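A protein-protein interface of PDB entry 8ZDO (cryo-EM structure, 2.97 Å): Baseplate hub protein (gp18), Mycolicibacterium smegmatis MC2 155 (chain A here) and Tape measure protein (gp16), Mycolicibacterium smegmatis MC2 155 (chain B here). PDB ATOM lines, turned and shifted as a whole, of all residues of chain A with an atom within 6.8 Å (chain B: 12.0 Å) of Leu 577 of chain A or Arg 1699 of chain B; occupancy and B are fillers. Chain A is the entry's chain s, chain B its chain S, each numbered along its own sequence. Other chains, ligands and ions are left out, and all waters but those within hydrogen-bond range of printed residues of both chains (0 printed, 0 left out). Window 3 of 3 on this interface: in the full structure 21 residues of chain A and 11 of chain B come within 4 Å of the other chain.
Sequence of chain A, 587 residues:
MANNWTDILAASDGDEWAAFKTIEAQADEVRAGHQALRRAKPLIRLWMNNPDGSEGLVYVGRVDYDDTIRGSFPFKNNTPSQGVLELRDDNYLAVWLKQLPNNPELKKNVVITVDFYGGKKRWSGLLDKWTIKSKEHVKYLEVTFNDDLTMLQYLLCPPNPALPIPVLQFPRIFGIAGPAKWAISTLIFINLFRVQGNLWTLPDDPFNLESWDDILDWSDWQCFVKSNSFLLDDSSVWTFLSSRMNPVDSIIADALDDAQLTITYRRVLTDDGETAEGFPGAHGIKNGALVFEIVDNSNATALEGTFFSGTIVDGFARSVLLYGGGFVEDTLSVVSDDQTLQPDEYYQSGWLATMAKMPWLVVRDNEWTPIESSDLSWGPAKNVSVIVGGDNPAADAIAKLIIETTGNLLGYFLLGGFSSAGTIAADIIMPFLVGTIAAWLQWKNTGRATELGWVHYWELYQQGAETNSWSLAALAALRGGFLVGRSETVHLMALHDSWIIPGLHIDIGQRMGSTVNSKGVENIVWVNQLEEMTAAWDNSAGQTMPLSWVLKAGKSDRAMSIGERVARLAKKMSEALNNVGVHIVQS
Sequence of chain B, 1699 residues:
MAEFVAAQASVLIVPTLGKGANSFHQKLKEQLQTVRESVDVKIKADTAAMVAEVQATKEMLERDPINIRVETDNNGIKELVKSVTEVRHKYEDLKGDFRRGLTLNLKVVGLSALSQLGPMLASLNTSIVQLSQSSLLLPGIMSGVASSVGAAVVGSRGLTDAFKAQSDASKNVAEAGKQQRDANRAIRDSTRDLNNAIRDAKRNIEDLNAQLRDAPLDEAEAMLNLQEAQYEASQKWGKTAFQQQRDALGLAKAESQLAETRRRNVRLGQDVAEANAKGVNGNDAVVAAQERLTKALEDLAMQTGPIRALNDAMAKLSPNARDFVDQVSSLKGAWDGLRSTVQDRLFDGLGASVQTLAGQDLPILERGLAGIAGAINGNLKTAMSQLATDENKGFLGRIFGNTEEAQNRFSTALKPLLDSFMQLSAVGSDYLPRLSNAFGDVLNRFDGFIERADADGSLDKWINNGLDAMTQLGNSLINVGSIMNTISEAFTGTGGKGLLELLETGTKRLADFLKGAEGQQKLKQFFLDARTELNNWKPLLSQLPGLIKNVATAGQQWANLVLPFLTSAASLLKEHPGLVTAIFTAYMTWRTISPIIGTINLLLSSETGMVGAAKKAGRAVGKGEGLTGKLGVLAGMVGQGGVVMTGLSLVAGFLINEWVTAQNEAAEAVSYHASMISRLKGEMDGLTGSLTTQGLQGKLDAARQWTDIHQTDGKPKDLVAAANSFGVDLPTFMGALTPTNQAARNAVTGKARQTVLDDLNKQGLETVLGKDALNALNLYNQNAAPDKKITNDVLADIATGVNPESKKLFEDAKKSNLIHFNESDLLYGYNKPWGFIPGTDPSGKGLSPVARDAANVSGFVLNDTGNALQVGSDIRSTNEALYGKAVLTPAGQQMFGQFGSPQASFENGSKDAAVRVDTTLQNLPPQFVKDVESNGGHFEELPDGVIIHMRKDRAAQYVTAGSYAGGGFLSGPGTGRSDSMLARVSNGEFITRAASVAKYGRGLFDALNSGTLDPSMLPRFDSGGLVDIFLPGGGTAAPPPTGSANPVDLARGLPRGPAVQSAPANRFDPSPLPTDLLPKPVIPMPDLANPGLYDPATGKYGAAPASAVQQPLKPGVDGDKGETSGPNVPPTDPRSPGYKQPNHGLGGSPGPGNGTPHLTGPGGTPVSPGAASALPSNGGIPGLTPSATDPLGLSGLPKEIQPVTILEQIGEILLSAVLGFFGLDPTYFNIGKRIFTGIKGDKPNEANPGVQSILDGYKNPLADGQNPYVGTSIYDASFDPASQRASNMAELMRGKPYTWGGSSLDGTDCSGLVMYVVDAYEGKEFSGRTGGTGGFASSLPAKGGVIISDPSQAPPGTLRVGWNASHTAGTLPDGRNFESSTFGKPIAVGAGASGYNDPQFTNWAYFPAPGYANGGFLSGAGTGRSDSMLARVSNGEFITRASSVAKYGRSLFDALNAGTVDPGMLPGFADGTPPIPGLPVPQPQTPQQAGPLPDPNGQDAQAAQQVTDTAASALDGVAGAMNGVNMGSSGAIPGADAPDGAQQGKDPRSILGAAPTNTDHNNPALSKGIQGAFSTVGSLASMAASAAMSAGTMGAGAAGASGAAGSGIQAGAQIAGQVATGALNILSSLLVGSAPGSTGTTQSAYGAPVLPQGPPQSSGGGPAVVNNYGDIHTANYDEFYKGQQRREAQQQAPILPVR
OD1 of Asn 578 of chain A lies within hydrogen-bond range of NH2 of Arg 1699 of chain B. The guanidinium group of Arg 1699 of chain B lies within hydrogen-bond range of the side-chain hydroxyl of Ser 574 of chain A, 3.0 Å away.
The backbone carbonyl oxygen (O) of Ser 574 of chain A sits close to the side-chain amide oxygen (OD1) of Asn 578 of chain A (3.4 Å).
Pro 1697 of chain B touches Ala 570 of chain A (CG to O, 3.7 Å). CB of Ser 574 of chain A touches CG of Pro 1697 of chain B, 3.9 Å away. CB of Leu 577 of chain A touches NH1 of Arg 1699 of chain B, 3.7 Å away.
Of the printed residues of chain B, Leu 577 of chain A touches Arg 1699 (3.7 Å). Arg 1699 of chain B touches just these residues of chain A: Ser 574 (3.0 Å), Leu 577 (3.7 Å) and Asn 578 (2.5 Å). Ser 574 of chain A touches two residues of chain B. No residue of chain B comes within 4 Å of Ala 576 of chain A. Of the printed residues of chain B, Asn 578 of chain A touches Arg 1699. No residue of chain B comes within 4 Å of Asn 579 of chain A. Val 580 of chain A touches none of the printed residues of chain B. Printed residues of chain A within 4 Å of Pro 1697 of chain B: Ala 570 and Ser 574. Of the printed residues of chain B, Ala 570 of chain A touches Pro 1697 (3.7 Å). The nearest residue of chain B that does not touch Leu 577 of chain A is Pro 1697 of chain B (9.5 Å). The nearest residue of chain A that does not touch Arg 1699 of chain B is Met 573 of chain A (4.9 Å).
Printed residues of chain B that touch a printed residue of chain A: Pro 1697 and Arg 1699. Hydrophobic or aromatic side chains of chain B that line the printed part of chain A: Pro 1697. Along chain B the printed residues that touch a printed residue of chain A span positions 1697 to 1699. Of the 14 printed residues of chain A, 4 touch a printed residue of chain B. Among the printed residues, no Asp or Glu carboxylate lies within 4 Å of a Lys or Arg side-chain nitrogen of the other chain.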
ATOM      1  N   GLN A 463       2.102 -22.268 -13.447  1.00  0.00           N
ATOM      2  CA  GLN A 463       1.691 -23.618 -13.097  1.00  0.00           C
ATOM      3  C   GLN A 463       0.212 -23.601 -12.736  1.00  0.00           C
ATOM      4  O   GLN A 463      -0.213 -22.815 -11.885  1.00  0.00           O
ATOM      5  CB  GLN A 463       2.518 -24.150 -11.927  1.00  0.00           C
ATOM      6  CG  GLN A 463       2.648 -25.656 -11.880  1.00  0.00           C
ATOM      7  CD  GLN A 463       3.220 -26.139 -10.568  1.00  0.00           C
ATOM      8  OE1 GLN A 463       3.172 -25.433  -9.563  1.00  0.00           O
ATOM      9  NE2 GLN A 463       3.775 -27.343 -10.570  1.00  0.00           N
ATOM     10  N   ALA A 570       0.785 -18.941   0.232  1.00  0.00           N
ATOM     11  CA  ALA A 570       0.899 -20.183   0.983  1.00  0.00           C
ATOM     12  C   ALA A 570      -0.235 -21.132   0.638  1.00  0.00           C
ATOM     13  O   ALA A 570      -0.025 -22.342   0.512  1.00  0.00           O
ATOM     14  CB  ALA A 570       0.919 -19.889   2.481  1.00  0.00           C
ATOM     15  N   LYS A 572      -1.911 -21.283  -2.260  1.00  0.00           N
ATOM     16  CA  LYS A 572      -1.668 -21.823  -3.592  1.00  0.00           C
ATOM     17  C   LYS A 572      -0.528 -22.833  -3.581  1.00  0.00           C
ATOM     18  O   LYS A 572      -0.606 -23.875  -4.241  1.00  0.00           O
ATOM     19  CB  LYS A 572      -1.373 -20.691  -4.573  1.00  0.00           C
ATOM     20  CG  LYS A 572      -2.618 -20.028  -5.131  1.00  0.00           C
ATOM     21  CD  LYS A 572      -2.272 -18.769  -5.903  1.00  0.00           C
ATOM     22  CE  LYS A 572      -1.673 -17.714  -4.991  1.00  0.00           C
ATOM     23  NZ  LYS A 572      -1.679 -16.369  -5.622  1.00  0.00           N
ATOM     24  N   MET A 573       0.538 -22.544  -2.832  1.00  0.00           N
ATOM     25  CA  MET A 573       1.676 -23.451  -2.773  1.00  0.00           C
ATOM     26  C   MET A 573       1.312 -24.763  -2.095  1.00  0.00           C
ATOM     27  O   MET A 573       1.764 -25.828  -2.521  1.00  0.00           O
ATOM     28  CB  MET A 573       2.844 -22.780  -2.055  1.00  0.00           C
ATOM     29  CG  MET A 573       3.713 -21.926  -2.958  1.00  0.00           C
ATOM     30  SD  MET A 573       4.675 -20.720  -2.035  1.00  0.00           S
ATOM     31  CE  MET A 573       5.247 -21.732  -0.680  1.00  0.00           C
ATOM     32  N   SER A 574       0.501 -24.712  -1.036  1.00  0.00           N
ATOM     33  CA  SER A 574       0.068 -25.943  -0.382  1.00  0.00           C
ATOM     34  C   SER A 574      -0.795 -26.785  -1.313  1.00  0.00           C
ATOM     35  O   SER A 574      -0.623 -28.010  -1.394  1.00  0.00           O
ATOM     36  CB  SER A 574      -0.688 -25.611   0.903  1.00  0.00           C
ATOM     37  OG  SER A 574      -1.004 -26.786   1.626  1.00  0.00           O
ATOM     38  N   GLU A 575      -1.722 -26.148  -2.032  1.00  0.00           N
ATOM     39  CA  GLU A 575      -2.545 -26.895  -2.980  1.00  0.00           C
ATOM     40  C   GLU A 575      -1.694 -27.516  -4.082  1.00  0.00           C
ATOM     41  O   GLU A 575      -1.892 -28.681  -4.454  1.00  0.00           O
ATOM     42  CB  GLU A 575      -3.616 -25.987  -3.575  1.00  0.00           C
ATOM     43  CG  GLU A 575      -4.628 -25.480  -2.563  1.00  0.00           C
ATOM     44  CD  GLU A 575      -5.381 -24.260  -3.056  1.00  0.00           C
ATOM     45  OE1 GLU A 575      -4.886 -23.590  -3.985  1.00  0.00           O
ATOM     46  OE2 GLU A 575      -6.468 -23.970  -2.512  1.00  0.00           O
ATOM     47  N   ALA A 576      -0.731 -26.756  -4.609  1.00  0.00           N
ATOM     48  CA  ALA A 576       0.124 -27.276  -5.669  1.00  0.00           C
ATOM     49  C   ALA A 576       1.018 -28.398  -5.162  1.00  0.00           C
ATOM     50  O   ALA A 576       1.295 -29.355  -5.891  1.00  0.00           O
ATOM     51  CB  ALA A 576       0.959 -26.148  -6.270  1.00  0.00           C
ATOM     52  N   LEU A 577       1.489 -28.291  -3.919  1.00  0.00           N
ATOM     53  CA  LEU A 577       2.288 -29.357  -3.329  1.00  0.00           C
ATOM     54  C   LEU A 577       1.474 -30.633  -3.180  1.00  0.00           C
ATOM     55  O   LEU A 577       1.964 -31.728  -3.477  1.00  0.00           O
ATOM     56  CB  LEU A 577       2.835 -28.904  -1.977  1.00  0.00           C
ATOM     57  CG  LEU A 577       4.010 -29.662  -1.365  1.00  0.00           C
ATOM     58  CD1 LEU A 577       5.043 -30.016  -2.416  1.00  0.00           C
ATOM     59  CD2 LEU A 577       4.631 -28.825  -0.268  1.00  0.00           C
ATOM     60  N   ASN A 578       0.222 -30.511  -2.732  1.00  0.00           N
ATOM     61  CA  ASN A 578      -0.646 -31.682  -2.655  1.00  0.00           C
ATOM     62  C   ASN A 578      -0.853 -32.299  -4.032  1.00  0.00           C
ATOM     63  O   ASN A 578      -0.796 -33.526  -4.189  1.00  0.00           O
ATOM     64  CB  ASN A 578      -1.989 -31.304  -2.037  1.00  0.00           C
ATOM     65  CG  ASN A 578      -1.891 -31.030  -0.557  1.00  0.00           C
ATOM     66  OD1 ASN A 578      -0.807 -31.060   0.020  1.00  0.00           O
ATOM     67  ND2 ASN A 578      -3.027 -30.756   0.070  1.00  0.00           N
ATOM     68  N   ASN A 579      -1.085 -31.462  -5.045  1.00  0.00           N
ATOM     69  CA  ASN A 579      -1.313 -31.978  -6.392  1.00  0.00           C
ATOM     70  C   ASN A 579      -0.077 -32.684  -6.939  1.00  0.00           C
ATOM     71  O   ASN A 579      -0.181 -33.758  -7.543  1.00  0.00           O
ATOM     72  CB  ASN A 579      -1.737 -30.843  -7.317  1.00  0.00           C
ATOM     73  CG  ASN A 579      -2.722 -31.292  -8.367  1.00  0.00           C
ATOM     74  OD1 ASN A 579      -3.360 -32.335  -8.233  1.00  0.00           O
ATOM     75  ND2 ASN A 579      -2.847 -30.510  -9.427  1.00  0.00           N
ATOM     76  N   VAL A 580       1.102 -32.099  -6.743  1.00  0.00           N
ATOM     77  CA  VAL A 580       2.322 -32.738  -7.224  1.00  0.00           C
ATOM     78  C   VAL A 580       2.557 -34.052  -6.492  1.00  0.00           C
ATOM     79  O   VAL A 580       2.870 -35.078  -7.111  1.00  0.00           O
ATOM     80  CB  VAL A 580       3.516 -31.779  -7.077  1.00  0.00           C
ATOM     81  CG1 VAL A 580       4.814 -32.543  -7.172  1.00  0.00           C
ATOM     82  CG2 VAL A 580       3.451 -30.693  -8.136  1.00  0.00           C
ATOM     83  N   GLY A 581       2.389 -34.052  -5.168  1.00  0.00           N
ATOM     84  CA  GLY A 581       2.579 -35.269  -4.404  1.00  0.00           C
ATOM     85  C   GLY A 581       1.632 -36.377  -4.809  1.00  0.00           C
ATOM     86  O   GLY A 581       2.004 -37.552  -4.797  1.00  0.00           O
ATOM     87  N   VAL A 582       0.399 -36.025  -5.173  1.00  0.00           N
ATOM     88  CA  VAL A 582      -0.531 -37.056  -5.617  1.00  0.00           C
ATOM     89  C   VAL A 582      -0.261 -37.471  -7.060  1.00  0.00           C
ATOM     90  O   VAL A 582      -0.631 -38.583  -7.457  1.00  0.00           O
ATOM     91  CB  VAL A 582      -1.985 -36.593  -5.424  1.00  0.00           C
ATOM     92  CG1 VAL A 582      -2.343 -35.483  -6.378  1.00  0.00           C
ATOM     93  CG2 VAL A 582      -2.924 -37.743  -5.585  1.00  0.00           C
ATOM     94  N   HIS A 583       0.393 -36.625  -7.851  1.00  0.00           N
ATOM     95  CA  HIS A 583       0.798 -37.005  -9.199  1.00  0.00           C
ATOM     96  C   HIS A 583       2.148 -37.711  -9.245  1.00  0.00           C
ATOM     97  O   HIS A 583       2.583 -38.108 -10.330  1.00  0.00           O
ATOM     98  CB  HIS A 583       0.830 -35.774 -10.109  1.00  0.00           C
ATOM     99  CG  HIS A 583      -0.519 -35.356 -10.601  1.00  0.00           C
ATOM    100  ND1 HIS A 583      -1.287 -36.150 -11.424  1.00  0.00           N
ATOM    101  CD2 HIS A 583      -1.236 -34.229 -10.387  1.00  0.00           C
ATOM    102  CE1 HIS A 583      -2.421 -35.531 -11.697  1.00  0.00           C
ATOM    103  NE2 HIS A 583      -2.417 -34.363 -11.079  1.00  0.00           N
ATOM    104  N   GLN B1692      -6.648 -12.752   7.139  1.00  0.00           N
ATOM    105  CA  GLN B1692      -5.804 -13.804   6.582  1.00  0.00           C
ATOM    106  C   GLN B1692      -6.125 -15.209   7.075  1.00  0.00           C
ATOM    107  O   GLN B1692      -5.706 -16.176   6.433  1.00  0.00           O
ATOM    108  CB  GLN B1692      -4.332 -13.510   6.887  1.00  0.00           C
ATOM    109  CG  GLN B1692      -3.791 -12.291   6.172  1.00  0.00           C
ATOM    110  CD  GLN B1692      -2.893 -11.453   7.053  1.00  0.00           C
ATOM    111  OE1 GLN B1692      -2.015 -11.976   7.737  1.00  0.00           O
ATOM    112  NE2 GLN B1692      -3.108 -10.144   7.041  1.00  0.00           N
ATOM    113  N   ALA B1693      -6.833 -15.353   8.190  1.00  0.00           N
ATOM    114  CA  ALA B1693      -7.076 -16.684   8.749  1.00  0.00           C
ATOM    115  C   ALA B1693      -7.891 -17.587   7.833  1.00  0.00           C
ATOM    116  O   ALA B1693      -7.497 -18.752   7.648  1.00  0.00           O
ATOM    117  CB  ALA B1693      -7.730 -16.548  10.126  1.00  0.00           C
ATOM    118  N   PRO B1694      -9.018 -17.157   7.250  1.00  0.00           N
ATOM    119  CA  PRO B1694      -9.781 -18.082   6.396  1.00  0.00           C
ATOM    120  C   PRO B1694      -9.010 -18.584   5.188  1.00  0.00           C
ATOM    121  O   PRO B1694      -9.242 -19.714   4.745  1.00  0.00           O
ATOM    122  CB  PRO B1694     -11.003 -17.251   5.982  1.00  0.00           C
ATOM    123  CG  PRO B1694     -10.572 -15.845   6.144  1.00  0.00           C
ATOM    124  CD  PRO B1694      -9.696 -15.852   7.348  1.00  0.00           C
ATOM    125  N   ILE B1695      -8.095 -17.782   4.634  1.00  0.00           N
ATOM    126  CA  ILE B1695      -7.365 -18.194   3.439  1.00  0.00           C
ATOM    127  C   ILE B1695      -6.094 -18.967   3.757  1.00  0.00           C
ATOM    128  O   ILE B1695      -5.448 -19.480   2.831  1.00  0.00           O
ATOM    129  CB  ILE B1695      -7.026 -16.978   2.556  1.00  0.00           C
ATOM    130  CG1 ILE B1695      -6.002 -16.081   3.243  1.00  0.00           C
ATOM    131  CG2 ILE B1695      -8.285 -16.190   2.239  1.00  0.00           C
ATOM    132  CD1 ILE B1695      -5.703 -14.815   2.480  1.00  0.00           C
ATOM    133  N   LEU B1696      -5.710 -19.065   5.023  1.00  0.00           N
ATOM    134  CA  LEU B1696      -4.559 -19.879   5.380  1.00  0.00           C
ATOM    135  C   LEU B1696      -4.917 -21.361   5.283  1.00  0.00           C
ATOM    136  O   LEU B1696      -5.989 -21.773   5.738  1.00  0.00           O
ATOM    137  CB  LEU B1696      -4.078 -19.546   6.790  1.00  0.00           C
ATOM    138  CG  LEU B1696      -3.053 -18.417   6.878  1.00  0.00           C
ATOM    139  CD1 LEU B1696      -2.691 -18.138   8.323  1.00  0.00           C
ATOM    140  CD2 LEU B1696      -1.814 -18.756   6.069  1.00  0.00           C
ATOM    141  N   PRO B1697      -4.048 -22.179   4.699  1.00  0.00           N
ATOM    142  CA  PRO B1697      -4.356 -23.603   4.540  1.00  0.00           C
ATOM    143  C   PRO B1697      -4.428 -24.329   5.872  1.00  0.00           C
ATOM    144  O   PRO B1697      -3.858 -23.914   6.882  1.00  0.00           O
ATOM    145  CB  PRO B1697      -3.194 -24.136   3.692  1.00  0.00           C
ATOM    146  CG  PRO B1697      -2.495 -22.950   3.177  1.00  0.00           C
ATOM    147  CD  PRO B1697      -2.754 -21.822   4.109  1.00  0.00           C
ATOM    148  N   VAL B1698      -5.156 -25.446   5.849  1.00  0.00           N
ATOM    149  CA  VAL B1698      -5.339 -26.259   7.045  1.00  0.00           C
ATOM    150  C   VAL B1698      -4.124 -27.129   7.346  1.00  0.00           C
ATOM    151  O   VAL B1698      -3.978 -27.599   8.481  1.00  0.00           O
ATOM    152  CB  VAL B1698      -6.598 -27.127   6.885  1.00  0.00           C
ATOM    153  CG1 VAL B1698      -6.350 -28.226   5.867  1.00  0.00           C
ATOM    154  CG2 VAL B1698      -7.046 -27.696   8.224  1.00  0.00           C
ATOM    155  N   ARG B1699      -3.246 -27.347   6.370  1.00  0.00           N
ATOM    156  CA  ARG B1699      -2.071 -28.193   6.559  1.00  0.00           C
ATOM    157  C   ARG B1699      -1.188 -27.682   7.690  1.00  0.00           C
ATOM    158  O   ARG B1699      -1.255 -28.179   8.813  1.00  0.00           O
ATOM    159  CB  ARG B1699      -1.258 -28.281   5.265  1.00  0.00           C
ATOM    160  CG  ARG B1699       0.239 -28.442   5.490  1.00  0.00           C
ATOM    161  CD  ARG B1699       1.011 -28.381   4.183  1.00  0.00           C
ATOM    162  NE  ARG B1699       1.014 -29.664   3.492  1.00  0.00           N
ATOM    163  CZ  ARG B1699       1.122 -29.807   2.179  1.00  0.00           C
ATOM    164  NH1 ARG B1699       1.235 -28.762   1.378  1.00  0.00           N
ATOM    165  NH2 ARG B1699       1.112 -31.029   1.657  1.00  0.00           N
